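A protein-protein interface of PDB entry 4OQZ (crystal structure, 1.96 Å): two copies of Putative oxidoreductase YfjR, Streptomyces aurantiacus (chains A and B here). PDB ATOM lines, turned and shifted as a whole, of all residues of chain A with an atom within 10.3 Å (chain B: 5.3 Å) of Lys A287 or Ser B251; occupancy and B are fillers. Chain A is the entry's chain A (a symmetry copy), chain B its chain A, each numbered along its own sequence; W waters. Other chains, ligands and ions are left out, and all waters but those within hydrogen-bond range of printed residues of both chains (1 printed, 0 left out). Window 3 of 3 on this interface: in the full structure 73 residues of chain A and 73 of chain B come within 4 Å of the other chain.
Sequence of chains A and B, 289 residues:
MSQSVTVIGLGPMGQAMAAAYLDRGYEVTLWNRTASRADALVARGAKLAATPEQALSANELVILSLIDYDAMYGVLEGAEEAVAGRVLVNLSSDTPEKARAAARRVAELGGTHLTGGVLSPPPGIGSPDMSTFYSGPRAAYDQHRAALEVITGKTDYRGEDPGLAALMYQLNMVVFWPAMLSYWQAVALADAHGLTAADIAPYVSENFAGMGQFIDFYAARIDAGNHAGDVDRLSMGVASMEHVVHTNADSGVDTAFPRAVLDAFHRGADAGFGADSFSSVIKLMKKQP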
ATOM      1  N   THR A  95      -0.360   1.206 -32.680  1.00  0.00           N
ATOM      2  CA  THR A  95      -0.259   2.300 -31.707  1.00  0.00           C
ATOM      3  C   THR A  95       0.953   3.230 -31.897  1.00  0.00           C
ATOM      4  O   THR A  95       1.998   2.762 -32.366  1.00  0.00           O
ATOM      5  CB  THR A  95      -0.245   1.744 -30.277  1.00  0.00           C
ATOM      6  OG1 THR A  95       0.985   1.055 -30.026  1.00  0.00           O
ATOM      7  CG2 THR A  95      -1.451   0.893 -29.961  1.00  0.00           C
ATOM      8  N   PRO A  96       0.869   4.508 -31.416  1.00  0.00           N
ATOM      9  CA  PRO A  96       2.038   5.412 -31.470  1.00  0.00           C
ATOM     10  C   PRO A  96       3.280   4.880 -30.763  1.00  0.00           C
ATOM     11  O   PRO A  96       4.385   5.143 -31.227  1.00  0.00           O
ATOM     12  CB  PRO A  96       1.535   6.691 -30.797  1.00  0.00           C
ATOM     13  CG  PRO A  96       0.068   6.641 -30.910  1.00  0.00           C
ATOM     14  CD  PRO A  96      -0.302   5.197 -30.833  1.00  0.00           C
ATOM     15  N   GLU A  97       3.105   4.135 -29.655  1.00  0.00           N
ATOM     16  CA  GLU A  97       4.212   3.549 -28.892  1.00  0.00           C
ATOM     17  C   GLU A  97       4.966   2.485 -29.700  1.00  0.00           C
ATOM     18  O   GLU A  97       6.192   2.542 -29.790  1.00  0.00           O
ATOM     19  CB  GLU A  97       3.731   3.021 -27.527  1.00  0.00           C
ATOM     20  CG  GLU A  97       4.592   3.463 -26.354  1.00  0.00           C
ATOM     21  CD  GLU A  97       4.817   4.956 -26.184  1.00  0.00           C
ATOM     22  OE1 GLU A  97       3.822   5.704 -26.045  1.00  0.00           O
ATOM     23  OE2 GLU A  97       5.996   5.376 -26.193  1.00  0.00           O
ATOM     24  N   ARG A 100       7.038   4.145 -32.420  1.00  0.00           N
ATOM     25  CA  ARG A 100       8.254   4.719 -31.849  1.00  0.00           C
ATOM     26  C   ARG A 100       9.300   3.636 -31.615  1.00  0.00           C
ATOM     27  O   ARG A 100      10.490   3.915 -31.789  1.00  0.00           O
ATOM     28  CB  ARG A 100       7.993   5.481 -30.524  1.00  0.00           C
ATOM     29  CG  ARG A 100       7.221   6.787 -30.702  1.00  0.00           C
ATOM     30  CD  ARG A 100       7.047   7.560 -29.400  1.00  0.00           C
ATOM     31  NE  ARG A 100       6.025   8.603 -29.536  1.00  0.00           N
ATOM     32  CZ  ARG A 100       4.807   8.549 -29.002  1.00  0.00           C
ATOM     33  NH1 ARG A 100       4.446   7.514 -28.253  1.00  0.00           N
ATOM     34  NH2 ARG A 100       3.949   9.541 -29.193  1.00  0.00           N
ATOM     35  N   ASP A 161       8.203  13.137 -34.880  1.00  0.00           N
ATOM     36  CA  ASP A 161       7.835  12.057 -33.967  1.00  0.00           C
ATOM     37  C   ASP A 161       7.221  10.835 -34.674  1.00  0.00           C
ATOM     38  O   ASP A 161       6.147  10.950 -35.259  1.00  0.00           O
ATOM     39  CB  ASP A 161       6.968  12.569 -32.791  1.00  0.00           C
ATOM     40  CG  ASP A 161       6.316  11.501 -31.917  1.00  0.00           C
ATOM     41  OD1 ASP A 161       6.955  10.454 -31.673  1.00  0.00           O
ATOM     42  OD2 ASP A 161       5.175  11.725 -31.459  1.00  0.00           O
ATOM     43  N   GLY A 163       5.495   8.387 -33.532  1.00  0.00           N
ATOM     44  CA  GLY A 163       4.149   8.127 -33.030  1.00  0.00           C
ATOM     45  C   GLY A 163       3.066   9.002 -33.621  1.00  0.00           C
ATOM     46  O   GLY A 163       1.894   8.622 -33.595  1.00  0.00           O
ATOM     47  N   ALA A 166       0.615   7.645 -36.449  1.00  0.00           N
ATOM     48  CA  ALA A 166      -0.128   6.575 -35.784  1.00  0.00           C
ATOM     49  C   ALA A 166      -1.208   7.182 -34.905  1.00  0.00           C
ATOM     50  O   ALA A 166      -2.323   6.693 -34.912  1.00  0.00           O
ATOM     51  CB  ALA A 166       0.818   5.722 -34.937  1.00  0.00           C
ATOM     52  N   LEU A 167      -0.874   8.254 -34.149  1.00  0.00           N
ATOM     53  CA  LEU A 167      -1.805   8.977 -33.293  1.00  0.00           C
ATOM     54  C   LEU A 167      -2.948   9.488 -34.159  1.00  0.00           C
ATOM     55  O   LEU A 167      -4.100   9.131 -33.911  1.00  0.00           O
ATOM     56  CB  LEU A 167      -1.062  10.161 -32.634  1.00  0.00           C
ATOM     57  CG  LEU A 167      -1.481  10.659 -31.270  1.00  0.00           C
ATOM     58  CD1 LEU A 167      -1.011  12.087 -31.108  1.00  0.00           C
ATOM     59  CD2 LEU A 167      -2.997  10.616 -31.043  1.00  0.00           C
ATOM     60  N   GLN A 170      -5.213   6.789 -35.183  1.00  0.00           N
ATOM     61  CA  GLN A 170      -6.116   6.388 -34.089  1.00  0.00           C
ATOM     62  C   GLN A 170      -7.238   7.402 -33.854  1.00  0.00           C
ATOM     63  O   GLN A 170      -8.382   7.007 -33.625  1.00  0.00           O
ATOM     64  CB  GLN A 170      -5.359   6.070 -32.784  1.00  0.00           C
ATOM     65  CG  GLN A 170      -4.255   5.007 -32.900  1.00  0.00           C
ATOM     66  CD  GLN A 170      -4.713   3.660 -33.412  1.00  0.00           C
ATOM     67  OE1 GLN A 170      -5.863   3.249 -33.255  1.00  0.00           O
ATOM     68  NE2 GLN A 170      -3.818   2.953 -34.066  1.00  0.00           N
ATOM     69  N   LEU A 171      -6.911   8.706 -33.988  1.00  0.00           N
ATOM     70  CA  LEU A 171      -7.832   9.828 -33.815  1.00  0.00           C
ATOM     71  C   LEU A 171      -8.949   9.695 -34.821  1.00  0.00           C
ATOM     72  O   LEU A 171     -10.116   9.892 -34.478  1.00  0.00           O
ATOM     73  CB  LEU A 171      -7.079  11.166 -33.970  1.00  0.00           C
ATOM     74  CG  LEU A 171      -6.904  12.105 -32.757  1.00  0.00           C
ATOM     75  CD1 LEU A 171      -7.191  11.432 -31.405  1.00  0.00           C
ATOM     76  CD2 LEU A 171      -5.541  12.740 -32.751  1.00  0.00           C
ATOM     77  N   VAL A 174     -11.118   6.561 -33.730  1.00  0.00           N
ATOM     78  CA  VAL A 174     -11.868   6.990 -32.539  1.00  0.00           C
ATOM     79  C   VAL A 174     -13.245   7.522 -32.941  1.00  0.00           C
ATOM     80  O   VAL A 174     -14.206   7.378 -32.220  1.00  0.00           O
ATOM     81  CB  VAL A 174     -11.056   8.041 -31.731  1.00  0.00           C
ATOM     82  CG1 VAL A 174     -11.945   9.054 -31.023  1.00  0.00           C
ATOM     83  CG2 VAL A 174     -10.134   7.368 -30.733  1.00  0.00           C
ATOM     84  N   VAL A 281     -17.622  16.734 -19.820  1.00  0.00           N
ATOM     85  CA  VAL A 281     -17.116  15.383 -19.598  1.00  0.00           C
ATOM     86  C   VAL A 281     -15.648  15.177 -20.017  1.00  0.00           C
ATOM     87  O   VAL A 281     -14.989  14.305 -19.460  1.00  0.00           O
ATOM     88  CB  VAL A 281     -18.064  14.226 -19.988  1.00  0.00           C
ATOM     89  CG1 VAL A 281     -18.515  13.460 -18.758  1.00  0.00           C
ATOM     90  CG2 VAL A 281     -19.260  14.712 -20.796  1.00  0.00           C
ATOM     91  N   ILE A 282     -15.120  16.002 -20.956  1.00  0.00           N
ATOM     92  CA  ILE A 282     -13.705  15.927 -21.386  1.00  0.00           C
ATOM     93  C   ILE A 282     -12.750  15.922 -20.173  1.00  0.00           C
ATOM     94  O   ILE A 282     -11.822  15.105 -20.133  1.00  0.00           O
ATOM     95  CB  ILE A 282     -13.322  17.043 -22.407  1.00  0.00           C
ATOM     96  CG1 ILE A 282     -14.058  16.852 -23.746  1.00  0.00           C
ATOM     97  CG2 ILE A 282     -11.799  17.089 -22.646  1.00  0.00           C
ATOM     98  CD1 ILE A 282     -14.072  18.045 -24.605  1.00  0.00           C
ATOM     99  N   LYS A 283     -12.987  16.824 -19.188  1.00  0.00           N
ATOM    100  CA  LYS A 283     -12.151  16.918 -17.978  1.00  0.00           C
ATOM    101  C   LYS A 283     -12.096  15.632 -17.129  1.00  0.00           C
ATOM    102  O   LYS A 283     -11.149  15.450 -16.364  1.00  0.00           O
ATOM    103  CB  LYS A 283     -12.312  18.233 -17.172  1.00  0.00           C
ATOM    104  CG  LYS A 283     -13.734  18.690 -16.883  1.00  0.00           C
ATOM    105  CD  LYS A 283     -13.858  20.213 -16.897  1.00  0.00           C
ATOM    106  CE  LYS A 283     -14.475  20.769 -15.630  1.00  0.00           C
ATOM    107  NZ  LYS A 283     -15.962  20.863 -15.693  1.00  0.00           N
ATOM    108  N   LEU A 284     -13.043  14.695 -17.366  1.00  0.00           N
ATOM    109  CA  LEU A 284     -13.049  13.377 -16.736  1.00  0.00           C
ATOM    110  C   LEU A 284     -12.334  12.351 -17.616  1.00  0.00           C
ATOM    111  O   LEU A 284     -11.896  11.324 -17.101  1.00  0.00           O
ATOM    112  CB  LEU A 284     -14.471  12.893 -16.446  1.00  0.00           C
ATOM    113  CG  LEU A 284     -15.244  13.618 -15.367  1.00  0.00           C
ATOM    114  CD1 LEU A 284     -16.677  13.244 -15.432  1.00  0.00           C
ATOM    115  CD2 LEU A 284     -14.695  13.298 -13.952  1.00  0.00           C
ATOM    116  N   MET A 285     -12.214  12.619 -18.935  1.00  0.00           N
ATOM    117  CA  MET A 285     -11.556  11.702 -19.877  1.00  0.00           C
ATOM    118  C   MET A 285     -10.049  11.883 -19.978  1.00  0.00           C
ATOM    119  O   MET A 285      -9.348  10.892 -20.168  1.00  0.00           O
ATOM    120  CB  MET A 285     -12.186  11.743 -21.277  1.00  0.00           C
ATOM    121  CG  MET A 285     -13.604  11.283 -21.317  1.00  0.00           C
ATOM    122  SD  MET A 285     -14.363  12.032 -22.758  1.00  0.00           S
ATOM    123  CE  MET A 285     -15.898  12.442 -22.108  1.00  0.00           C
ATOM    124  N   LYS A 286      -9.551  13.128 -19.871  1.00  0.00           N
ATOM    125  CA  LYS A 286      -8.113  13.454 -19.951  1.00  0.00           C
ATOM    126  C   LYS A 286      -7.277  12.753 -18.882  1.00  0.00           C
ATOM    127  O   LYS A 286      -7.823  12.376 -17.839  1.00  0.00           O
ATOM    128  CB  LYS A 286      -7.891  14.969 -19.837  1.00  0.00           C
ATOM    129  CG  LYS A 286      -8.484  15.794 -20.971  1.00  0.00           C
ATOM    130  CD  LYS A 286      -8.751  17.216 -20.491  1.00  0.00           C
ATOM    131  CE  LYS A 286      -7.648  18.198 -20.801  1.00  0.00           C
ATOM    132  NZ  LYS A 286      -7.873  18.872 -22.107  1.00  0.00           N
ATOM    133  N   LYS A 287      -5.948  12.607 -19.120  1.00  0.00           N
ATOM    134  CA  LYS A 287      -5.024  12.008 -18.143  1.00  0.00           C
ATOM    135  C   LYS A 287      -4.856  12.969 -16.966  1.00  0.00           C
ATOM    136  O   LYS A 287      -4.605  14.150 -17.192  1.00  0.00           O
ATOM    137  CB  LYS A 287      -3.646  11.699 -18.764  1.00  0.00           C
ATOM    138  CG  LYS A 287      -2.720  10.930 -17.809  1.00  0.00           C
ATOM    139  CD  LYS A 287      -1.270  10.888 -18.276  1.00  0.00           C
ATOM    140  CE  LYS A 287      -0.515   9.739 -17.650  1.00  0.00           C
ATOM    141  NZ  LYS A 287       0.828   9.556 -18.264  1.00  0.00           N
ATOM    142  N   LEU B 189      -7.635  12.471 -26.103  1.00  0.00           N
ATOM    143  CA  LEU B 189      -6.427  11.745 -26.508  1.00  0.00           C
ATOM    144  C   LEU B 189      -5.344  12.658 -27.096  1.00  0.00           C
ATOM    145  O   LEU B 189      -4.175  12.529 -26.744  1.00  0.00           O
ATOM    146  CB  LEU B 189      -6.753  10.573 -27.467  1.00  0.00           C
ATOM    147  CG  LEU B 189      -5.571   9.730 -27.969  1.00  0.00           C
ATOM    148  CD1 LEU B 189      -4.975   8.857 -26.859  1.00  0.00           C
ATOM    149  CD2 LEU B 189      -5.986   8.869 -29.127  1.00  0.00           C
ATOM    150  N   ALA B 192      -3.184  14.678 -24.448  1.00  0.00           N
ATOM    151  CA  ALA B 192      -2.045  13.955 -23.882  1.00  0.00           C
ATOM    152  C   ALA B 192      -0.852  13.885 -24.855  1.00  0.00           C
ATOM    153  O   ALA B 192       0.202  13.333 -24.501  1.00  0.00           O
ATOM    154  CB  ALA B 192      -2.470  12.559 -23.453  1.00  0.00           C
ATOM    155  N   HIS B 193      -1.010  14.504 -26.056  1.00  0.00           N
ATOM    156  CA  HIS B 193      -0.009  14.562 -27.123  1.00  0.00           C
ATOM    157  C   HIS B 193       0.311  15.967 -27.684  1.00  0.00           C
ATOM    158  O   HIS B 193       0.887  16.075 -28.765  1.00  0.00           O
ATOM    159  CB  HIS B 193      -0.386  13.593 -28.238  1.00  0.00           C
ATOM    160  CG  HIS B 193      -0.357  12.158 -27.821  1.00  0.00           C
ATOM    161  ND1 HIS B 193      -1.522  11.464 -27.558  1.00  0.00           N
ATOM    162  CD2 HIS B 193       0.696  11.321 -27.674  1.00  0.00           C
ATOM    163  CE1 HIS B 193      -1.145  10.233 -27.255  1.00  0.00           C
ATOM    164  NE2 HIS B 193       0.182  10.102 -27.301  1.00  0.00           N
ATOM    165  N   HIS B 246      -5.856   0.707 -26.751  1.00  0.00           N
ATOM    166  CA  HIS B 246      -4.475   0.702 -26.240  1.00  0.00           C
ATOM    167  C   HIS B 246      -3.831   2.084 -26.227  1.00  0.00           C
ATOM    168  O   HIS B 246      -3.262   2.467 -25.209  1.00  0.00           O
ATOM    169  CB  HIS B 246      -3.596  -0.345 -26.947  1.00  0.00           C
ATOM    170  CG  HIS B 246      -3.731  -1.729 -26.382  1.00  0.00           C
ATOM    171  ND1 HIS B 246      -3.008  -2.131 -25.267  1.00  0.00           N
ATOM    172  CD2 HIS B 246      -4.498  -2.763 -26.799  1.00  0.00           C
ATOM    173  CE1 HIS B 246      -3.358  -3.389 -25.046  1.00  0.00           C
ATOM    174  NE2 HIS B 246      -4.259  -3.811 -25.940  1.00  0.00           N
ATOM    175  N   THR B 247      -4.002   2.859 -27.314  1.00  0.00           N
ATOM    176  CA  THR B 247      -3.492   4.228 -27.485  1.00  0.00           C
ATOM    177  C   THR B 247      -3.981   5.145 -26.354  1.00  0.00           C
ATOM    178  O   THR B 247      -3.210   5.966 -25.842  1.00  0.00           O
ATOM    179  CB  THR B 247      -3.937   4.759 -28.866  1.00  0.00           C
ATOM    180  OG1 THR B 247      -3.461   3.886 -29.886  1.00  0.00           O
ATOM    181  CG2 THR B 247      -3.453   6.160 -29.149  1.00  0.00           C
ATOM    182  N   ASN B 248      -5.265   5.035 -26.006  1.00  0.00           N
ATOM    183  CA  ASN B 248      -5.885   5.834 -24.963  1.00  0.00           C
ATOM    184  C   ASN B 248      -5.382   5.388 -23.588  1.00  0.00           C
ATOM    185  O   ASN B 248      -5.057   6.232 -22.750  1.00  0.00           O
ATOM    186  CB  ASN B 248      -7.405   5.768 -25.067  1.00  0.00           C
ATOM    187  CG  ASN B 248      -7.950   6.598 -26.183  1.00  0.00           C
ATOM    188  OD1 ASN B 248      -8.168   7.801 -26.051  1.00  0.00           O
ATOM    189  ND2 ASN B 248      -8.162   5.982 -27.323  1.00  0.00           N
ATOM    190  N   ALA B 249      -5.254   4.060 -23.389  1.00  0.00           N
ATOM    191  CA  ALA B 249      -4.760   3.476 -22.137  1.00  0.00           C
ATOM    192  C   ALA B 249      -3.279   3.822 -21.918  1.00  0.00           C
ATOM    193  O   ALA B 249      -2.872   4.044 -20.778  1.00  0.00           O
ATOM    194  CB  ALA B 249      -4.960   1.967 -22.144  1.00  0.00           C
ATOM    195  N   ASP B 250      -2.485   3.888 -23.015  1.00  0.00           N
ATOM    196  CA  ASP B 250      -1.056   4.222 -22.967  1.00  0.00           C
ATOM    197  C   ASP B 250      -0.825   5.676 -22.543  1.00  0.00           C
ATOM    198  O   ASP B 250       0.157   5.956 -21.864  1.00  0.00           O
ATOM    199  CB  ASP B 250      -0.374   3.968 -24.327  1.00  0.00           C
ATOM    200  CG  ASP B 250      -0.137   2.515 -24.708  1.00  0.00           C
ATOM    201  OD1 ASP B 250      -0.200   1.642 -23.811  1.00  0.00           O
ATOM    202  OD2 ASP B 250       0.127   2.253 -25.903  1.00  0.00           O
ATOM    203  N   SER B 251      -1.722   6.587 -22.970  1.00  0.00           N
ATOM    204  CA  SER B 251      -1.675   8.019 -22.718  1.00  0.00           C
ATOM    205  C   SER B 251      -2.302   8.421 -21.375  1.00  0.00           C
ATOM    206  O   SER B 251      -2.278   9.598 -21.022  1.00  0.00           O
ATOM    207  CB  SER B 251      -2.378   8.758 -23.850  1.00  0.00           C
ATOM    208  OG  SER B 251      -1.934   8.303 -25.115  1.00  0.00           O
ATOM    209  N   GLY B 252      -2.855   7.452 -20.647  1.00  0.00           N
ATOM    210  CA  GLY B 252      -3.524   7.685 -19.371  1.00  0.00           C
ATOM    211  C   GLY B 252      -4.953   8.172 -19.534  1.00  0.00           C
ATOM    212  O   GLY B 252      -5.642   8.411 -18.539  1.00  0.00           O
ATOM    213  N   VAL B 253      -5.407   8.323 -20.797  1.00  0.00           N
ATOM    214  CA  VAL B 253      -6.751   8.780 -21.171  1.00  0.00           C
ATOM    215  C   VAL B 253      -7.767   7.662 -20.860  1.00  0.00           C
ATOM    216  O   VAL B 253      -7.437   6.484 -20.973  1.00  0.00           O
ATOM    217  CB  VAL B 253      -6.793   9.221 -22.677  1.00  0.00           C
ATOM    218  CG1 VAL B 253      -8.177   9.698 -23.096  1.00  0.00           C
ATOM    219  CG2 VAL B 253      -5.756  10.303 -22.968  1.00  0.00           C
HETATM  220  O   HOH W   1       0.711   0.098 -27.392  1.00  0.00           O
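O of Asn B248 sits at hydrogen-bond distance from N of Val B253 (2.9 Å). OG of Ser B251 lies within hydrogen-bond range of O of Thr B247 (2.8 Å). A ring nitrogen (ND1) of His B193 is in hydrogen-bond range of the backbone carbonyl oxygen of Leu B189 (3.0 Å).
CG2 of Thr A95 touches CB of His B246, 3.9 Å away. OG1 of Thr B247 touches CG2 of Thr A95, 3.6 Å away. Pro A96 touches Thr B247 (CD to OG1, 3.5 Å). Leu A167 touches Leu B189. CD1 of Leu A167 touches CB of His B193, 3.3 Å away. CG of Gln A170 touches OG1 of Thr B247, 3.3 Å away. Leu A171 touches Leu B189. CG1 of Val B253 touches O of Met A285, 3.4 Å away. Lys A287 touches Ser B251 (CD to O, 3.2 Å). Lys A287 touches Gly B252.
Of chain B, only Ser B251 and Gly B252 come within 4 Å of Lys A287. Ser B251 touches just one residue of chain A: Lys A287 (3.2 Å). No residue of chain A comes within 4 Å of Ala B249. Of the printed residues of chain A, Val B253 touches Met A285. Printed residues of chain A within 4 Å of His B246: Thr A95. Of the printed residues of chain A, Thr B247 touches Thr A95 (3.6 Å), Pro A96 (3.5 Å) and Gln A170 (3.3 Å). Of the printed residues of chain A, His B193 touches Leu A167 (3.3 Å). Of the printed residues of chain B, Leu A171 touches Leu B189 (3.6 Å). Of the printed residues of chain A, Leu B189 touches Leu A167 and Leu A171. Glu A97 touches none of the printed residues of chain B. Asp A161 touches none of the printed residues of chain B. The nearest residue of chain A that does not touch Ser B251 is Lys A286 (6.3 Å).
Hydrophobic or aromatic side chains of chain A within 4 Å of the printed part of chain B: Pro A96, Leu A167 and Leu A171. Of the 11 printed residues of chain B, 7 touch a printed residue of chain A. Printed residues of chain B that touch a printed residue of chain A: Leu B189, His B193, His B246, Thr B247, Ser B251, Gly B252 and Val B253. Along chain B the printed residues that touch a printed residue of chain A span positions 189 to 253. Among the printed residues, 10 pairs touch across the chains. Among the printed residues, no Asp or Glu carboxylate lies within 4 Å of a Lys or Arg side-chain nitrogen of the other chain.
No position is printed for both chains. Of the 10 pairs that touch across the chains among the printed residues, none has its exchanged pair printed and touching as well.
Water W1 bridges OD2 of Asp B250 (2.7 Å) and OG1 of Thr A95 (2.8 Å).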
